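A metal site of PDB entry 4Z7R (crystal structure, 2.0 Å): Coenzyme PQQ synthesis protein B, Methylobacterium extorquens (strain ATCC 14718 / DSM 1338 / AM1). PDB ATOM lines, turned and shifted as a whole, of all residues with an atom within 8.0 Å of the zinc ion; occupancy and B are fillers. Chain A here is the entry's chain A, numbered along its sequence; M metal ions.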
ATOM      1  N   GLY A  13      21.051  -1.434  -2.725  1.00  0.00           N
ATOM      2  CA  GLY A  13      20.473  -0.148  -3.059  1.00  0.00           C
ATOM      3  C   GLY A  13      21.112   1.005  -2.300  1.00  0.00           C
ATOM      4  O   GLY A  13      22.141   0.845  -1.648  1.00  0.00           O
ATOM      5  N   VAL A  14      20.503   2.180  -2.423  1.00  0.00           N
ATOM      6  CA  VAL A  14      20.945   3.369  -1.694  1.00  0.00           C
ATOM      7  C   VAL A  14      19.716   4.034  -1.075  1.00  0.00           C
ATOM      8  O   VAL A  14      18.835   4.474  -1.794  1.00  0.00           O
ATOM      9  CB  VAL A  14      21.683   4.375  -2.605  1.00  0.00           C
ATOM     10  CG1 VAL A  14      22.236   5.518  -1.772  1.00  0.00           C
ATOM     11  CG2 VAL A  14      22.807   3.696  -3.374  1.00  0.00           C
ATOM     12  N   PRO A  15      19.655   4.092   0.261  1.00  0.00           N
ATOM     13  CA  PRO A  15      20.641   3.506   1.185  1.00  0.00           C
ATOM     14  C   PRO A  15      20.493   1.999   1.304  1.00  0.00           C
ATOM     15  O   PRO A  15      19.491   1.430   0.857  1.00  0.00           O
ATOM     16  CB  PRO A  15      20.316   4.187   2.516  1.00  0.00           C
ATOM     17  CG  PRO A  15      18.824   4.389   2.438  1.00  0.00           C
ATOM     18  CD  PRO A  15      18.538   4.721   0.986  1.00  0.00           C
ATOM     19  N   GLN A  16      21.480   1.359   1.920  1.00  0.00           N
ATOM     20  CA  GLN A  16      21.391  -0.058   2.227  1.00  0.00           C
ATOM     21  C   GLN A  16      20.831  -0.210   3.638  1.00  0.00           C
ATOM     22  O   GLN A  16      21.152   0.574   4.530  1.00  0.00           O
ATOM     23  CB  GLN A  16      22.756  -0.721   2.097  1.00  0.00           C
ATOM     24  CG  GLN A  16      22.802  -2.192   2.465  1.00  0.00           C
ATOM     25  CD  GLN A  16      24.138  -2.811   2.146  1.00  0.00           C
ATOM     26  OE1 GLN A  16      24.584  -2.790   0.999  1.00  0.00           O
ATOM     27  NE2 GLN A  16      24.805  -3.333   3.163  1.00  0.00           N
ATOM     28  N   TRP A  17      19.961  -1.200   3.823  1.00  0.00           N
ATOM     29  CA  TRP A  17      19.108  -1.279   5.014  1.00  0.00           C
ATOM     30  C   TRP A  17      19.887  -1.311   6.332  1.00  0.00           C
ATOM     31  O   TRP A  17      19.373  -0.868   7.358  1.00  0.00           O
ATOM     32  CB  TRP A  17      18.193  -2.498   4.936  1.00  0.00           C
ATOM     33  CG  TRP A  17      18.892  -3.801   5.147  1.00  0.00           C
ATOM     34  CD1 TRP A  17      19.696  -4.460   4.253  1.00  0.00           C
ATOM     35  CD2 TRP A  17      18.843  -4.610   6.326  1.00  0.00           C
ATOM     36  NE1 TRP A  17      20.150  -5.638   4.816  1.00  0.00           N
ATOM     37  CE2 TRP A  17      19.637  -5.746   6.080  1.00  0.00           C
ATOM     38  CE3 TRP A  17      18.203  -4.482   7.568  1.00  0.00           C
ATOM     39  CZ2 TRP A  17      19.813  -6.752   7.031  1.00  0.00           C
ATOM     40  CZ3 TRP A  17      18.383  -5.487   8.506  1.00  0.00           C
ATOM     41  CH2 TRP A  17      19.170  -6.604   8.228  1.00  0.00           C
ATOM     42  N   ASN A  18      21.104  -1.840   6.297  1.00  0.00           N
ATOM     43  CA  ASN A  18      21.916  -1.910   7.513  1.00  0.00           C
ATOM     44  C   ASN A  18      23.209  -1.110   7.417  1.00  0.00           C
ATOM     45  O   ASN A  18      24.186  -1.408   8.091  1.00  0.00           O
ATOM     46  CB  ASN A  18      22.250  -3.367   7.831  1.00  0.00           C
ATOM     47  CG  ASN A  18      23.164  -3.993   6.804  1.00  0.00           C
ATOM     48  OD1 ASN A  18      23.200  -3.569   5.646  1.00  0.00           O
ATOM     49  ND2 ASN A  18      23.929  -5.005   7.218  1.00  0.00           N
ATOM     50  N   CYS A  19      23.219  -0.091   6.553  1.00  0.00           N
ATOM     51  CA  CYS A  19      24.428   0.697   6.375  1.00  0.00           C
ATOM     52  C   CYS A  19      24.271   2.134   6.829  1.00  0.00           C
ATOM     53  O   CYS A  19      23.261   2.774   6.535  1.00  0.00           O
ATOM     54  CB  CYS A  19      24.884   0.665   4.915  1.00  0.00           C
ATOM     55  SG  CYS A  19      26.494   1.430   4.659  1.00  0.00           S
ATOM     56  N   ARG A  20      25.273   2.635   7.537  1.00  0.00           N
ATOM     57  CA  ARG A  20      25.314   4.045   7.931  1.00  0.00           C
ATOM     58  C   ARG A  20      26.628   4.702   7.501  1.00  0.00           C
ATOM     59  O   ARG A  20      27.156   5.549   8.212  1.00  0.00           O
ATOM     60  CB  ARG A  20      25.137   4.191   9.439  1.00  0.00           C
ATOM     61  CG  ARG A  20      23.684   4.122   9.883  1.00  0.00           C
ATOM     62  CD  ARG A  20      22.909   5.333   9.404  1.00  0.00           C
ATOM     63  NE  ARG A  20      22.979   6.440  10.361  1.00  0.00           N
ATOM     64  CZ  ARG A  20      21.925   7.143  10.750  1.00  0.00           C
ATOM     65  NH1 ARG A  20      20.717   6.861  10.270  1.00  0.00           N
ATOM     66  NH2 ARG A  20      22.068   8.137  11.624  1.00  0.00           N
ATOM     67  N   CYS A  21      27.147   4.308   6.336  1.00  0.00           N
ATOM     68  CA  CYS A  21      28.281   5.012   5.756  1.00  0.00           C
ATOM     69  C   CYS A  21      27.882   6.451   5.459  1.00  0.00           C
ATOM     70  O   CYS A  21      26.707   6.805   5.563  1.00  0.00           O
ATOM     71  CB  CYS A  21      28.800   4.295   4.491  1.00  0.00           C
ATOM     72  SG  CYS A  21      27.894   4.581   2.927  1.00  0.00           S
ATOM     73  N   SER A  22      28.849   7.289   5.116  1.00  0.00           N
ATOM     74  CA  SER A  22      28.580   8.715   4.924  1.00  0.00           C
ATOM     75  C   SER A  22      27.569   8.974   3.802  1.00  0.00           C
ATOM     76  O   SER A  22      26.787   9.918   3.867  1.00  0.00           O
ATOM     77  CB  SER A  22      29.886   9.464   4.637  1.00  0.00           C
ATOM     78  OG  SER A  22      30.638   8.797   3.634  1.00  0.00           O
ATOM     79  N   ILE A  23      27.587   8.118   2.786  1.00  0.00           N
ATOM     80  CA  ILE A  23      26.656   8.265   1.666  1.00  0.00           C
ATOM     81  C   ILE A  23      25.240   7.858   2.061  1.00  0.00           C
ATOM     82  O   ILE A  23      24.294   8.628   1.861  1.00  0.00           O
ATOM     83  CB  ILE A  23      27.131   7.453   0.451  1.00  0.00           C
ATOM     84  CG1 ILE A  23      28.421   8.065  -0.108  1.00  0.00           C
ATOM     85  CG2 ILE A  23      26.058   7.432  -0.633  1.00  0.00           C
ATOM     86  CD1 ILE A  23      29.235   7.126  -0.977  1.00  0.00           C
ATOM     87  N   CYS A  24      25.098   6.658   2.612  1.00  0.00           N
ATOM     88  CA  CYS A  24      23.788   6.193   3.071  1.00  0.00           C
ATOM     89  C   CYS A  24      23.197   7.121   4.122  1.00  0.00           C
ATOM     90  O   CYS A  24      21.991   7.378   4.116  1.00  0.00           O
ATOM     91  CB  CYS A  24      23.888   4.771   3.631  1.00  0.00           C
ATOM     92  SG  CYS A  24      24.109   3.494   2.381  1.00  0.00           S
ATOM     93  N   SER A  25      24.034   7.625   5.020  1.00  0.00           N
ATOM     94  CA  SER A  25      23.580   8.509   6.087  1.00  0.00           C
ATOM     95  C   SER A  25      22.953   9.777   5.511  1.00  0.00           C
ATOM     96  O   SER A  25      21.974  10.289   6.056  1.00  0.00           O
ATOM     97  CB  SER A  25      24.739   8.881   7.018  1.00  0.00           C
ATOM     98  OG  SER A  25      25.211   7.726   7.693  1.00  0.00           O
ATOM     99  N   TRP A  28      19.549   8.618   4.354  1.00  0.00           N
ATOM    100  CA  TRP A  28      18.645   8.411   5.479  1.00  0.00           C
ATOM    101  C   TRP A  28      18.099   9.741   6.004  1.00  0.00           C
ATOM    102  O   TRP A  28      16.947   9.829   6.438  1.00  0.00           O
ATOM    103  CB  TRP A  28      19.344   7.672   6.628  1.00  0.00           C
ATOM    104  CG  TRP A  28      19.675   6.228   6.347  1.00  0.00           C
ATOM    105  CD1 TRP A  28      20.929   5.664   6.330  1.00  0.00           C
ATOM    106  CD2 TRP A  28      18.754   5.157   6.084  1.00  0.00           C
ATOM    107  NE1 TRP A  28      20.838   4.320   6.055  1.00  0.00           N
ATOM    108  CE2 TRP A  28      19.515   3.988   5.901  1.00  0.00           C
ATOM    109  CE3 TRP A  28      17.367   5.090   5.975  1.00  0.00           C
ATOM    110  CZ2 TRP A  28      18.937   2.757   5.617  1.00  0.00           C
ATOM    111  CZ3 TRP A  28      16.781   3.858   5.696  1.00  0.00           C
ATOM    112  CH2 TRP A  28      17.566   2.711   5.522  1.00  0.00           C
ATOM    113  N   MET A 225      34.869   0.046  -0.331  1.00  0.00           N
ATOM    114  CA  MET A 225      34.132  -0.433   0.821  1.00  0.00           C
ATOM    115  C   MET A 225      34.989  -0.326   2.081  1.00  0.00           C
ATOM    116  O   MET A 225      34.483  -0.062   3.171  1.00  0.00           O
ATOM    117  CB  MET A 225      33.677  -1.870   0.605  1.00  0.00           C
ATOM    118  CG  MET A 225      32.743  -2.057  -0.579  1.00  0.00           C
ATOM    119  SD  MET A 225      31.118  -2.650  -0.083  1.00  0.00           S
ATOM    120  CE  MET A 225      31.553  -4.210   0.694  1.00  0.00           C
ATOM    121  N   ALA A 228      35.164   3.272   3.060  1.00  0.00           N
ATOM    122  CA  ALA A 228      33.872   3.687   3.605  1.00  0.00           C
ATOM    123  C   ALA A 228      33.664   3.124   4.999  1.00  0.00           C
ATOM    124  O   ALA A 228      32.786   3.560   5.733  1.00  0.00           O
ATOM    125  CB  ALA A 228      32.747   3.259   2.685  1.00  0.00           C
ATOM    126  N   VAL A 230      32.768   0.003   5.798  1.00  0.00           N
ATOM    127  CA  VAL A 230      31.625  -0.909   5.897  1.00  0.00           C
ATOM    128  C   VAL A 230      31.979  -2.361   5.616  1.00  0.00           C
ATOM    129  O   VAL A 230      31.179  -3.260   5.873  1.00  0.00           O
ATOM    130  CB  VAL A 230      30.499  -0.502   4.919  1.00  0.00           C
ATOM    131  CG1 VAL A 230      30.149   0.958   5.075  1.00  0.00           C
ATOM    132  CG2 VAL A 230      30.910  -0.801   3.488  1.00  0.00           C
ATOM    133  N   ASN A 267      27.439   0.938  -6.178  1.00  0.00           N
ATOM    134  CA  ASN A 267      27.284   0.573  -4.768  1.00  0.00           C
ATOM    135  C   ASN A 267      27.116   1.791  -3.883  1.00  0.00           C
ATOM    136  O   ASN A 267      27.579   2.881  -4.213  1.00  0.00           O
ATOM    137  CB  ASN A 267      28.476  -0.255  -4.282  1.00  0.00           C
ATOM    138  CG  ASN A 267      28.149  -1.046  -3.027  1.00  0.00           C
ATOM    139  OD1 ASN A 267      27.155  -1.770  -2.990  1.00  0.00           O
ATOM    140  ND2 ASN A 267      28.971  -0.915  -1.996  1.00  0.00           N
ATOM    141  N   ASN A 268      26.447   1.603  -2.751  1.00  0.00           N
ATOM    142  CA  ASN A 268      26.177   2.699  -1.830  1.00  0.00           C
ATOM    143  C   ASN A 268      27.439   3.380  -1.326  1.00  0.00           C
ATOM    144  O   ASN A 268      27.387   4.498  -0.823  1.00  0.00           O
ATOM    145  CB  ASN A 268      25.338   2.198  -0.639  1.00  0.00           C
ATOM    146  CG  ASN A 268      26.114   1.264   0.254  1.00  0.00           C
ATOM    147  OD1 ASN A 268      26.834   1.694   1.168  1.00  0.00           O
ATOM    148  ND2 ASN A 268      25.973  -0.045   0.022  1.00  0.00           N
ATOM    149  N   THR A 269      28.569   2.689  -1.442  1.00  0.00           N
ATOM    150  CA  THR A 269      29.851   3.211  -0.958  1.00  0.00           C
ATOM    151  C   THR A 269      30.613   4.037  -2.001  1.00  0.00           C
ATOM    152  O   THR A 269      31.726   4.486  -1.743  1.00  0.00           O
ATOM    153  CB  THR A 269      30.762   2.067  -0.504  1.00  0.00           C
ATOM    154  OG1 THR A 269      30.883   1.113  -1.562  1.00  0.00           O
ATOM    155  CG2 THR A 269      30.171   1.375   0.715  1.00  0.00           C
ATOM    156  N   ASN A 270      30.009   4.243  -3.171  1.00  0.00           N
ATOM    157  CA  ASN A 270      30.701   4.939  -4.249  1.00  0.00           C
ATOM    158  C   ASN A 270      30.443   6.439  -4.196  1.00  0.00           C
ATOM    159  O   ASN A 270      29.305   6.885  -4.315  1.00  0.00           O
ATOM    160  CB  ASN A 270      30.288   4.370  -5.601  1.00  0.00           C
ATOM    161  CG  ASN A 270      31.191   4.819  -6.741  1.00  0.00           C
ATOM    162  OD1 ASN A 270      31.729   5.921  -6.731  1.00  0.00           O
ATOM    163  ND2 ASN A 270      31.358   3.951  -7.728  1.00  0.00           N
ATOM    164  N   LEU A 273      28.079   8.923  -6.124  1.00  0.00           N
ATOM    165  CA  LEU A 273      26.686   9.072  -5.734  1.00  0.00           C
ATOM    166  C   LEU A 273      26.434  10.419  -5.084  1.00  0.00           C
ATOM    167  O   LEU A 273      25.314  10.929  -5.083  1.00  0.00           O
ATOM    168  CB  LEU A 273      26.263   7.954  -4.777  1.00  0.00           C
ATOM    169  CG  LEU A 273      26.185   6.538  -5.342  1.00  0.00           C
ATOM    170  CD1 LEU A 273      25.928   5.553  -4.218  1.00  0.00           C
ATOM    171  CD2 LEU A 273      25.106   6.446  -6.408  1.00  0.00           C
HETATM  172 ZN    ZN M   1      26.330   2.840   2.840  1.00  0.00          ZN
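OD1 of Asn 268 is bound to the zinc ion, 2.1 Å away.
The zinc ion is bound by SG of Cys 19, at 2.3 Å.
The side-chain sulfur (SG) of Cys 21 binds the zinc ion (2.3 Å).
SG of Cys 24 is bound to the zinc ion, at 2.4 Å.
O of Cys 21 lies within hydrogen-bond range of OG of Ser 25 (2.8 Å).
ND2 of Asn 268 is in hydrogen-bond range of OE1 of Gln 16.
N of Ile 23 sits close to SG of Cys 21 (3.6 Å).
The indole nitrogen of Trp 28 lies within hydrogen-bond range of the backbone carbonyl oxygen of Cys 19 (2.9 Å).
The backbone NH (N) of Gln 16 sits close to the side-chain sulfur (SG) of Cys 24 (3.4 Å).
Four residues have an atom within 4 Å of the zinc ion: Cys 19, Cys 21, Cys 24 and Asn 268.
The nearest printed residue that does not touch the zinc ion is Thr 269 (4.6 Å).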
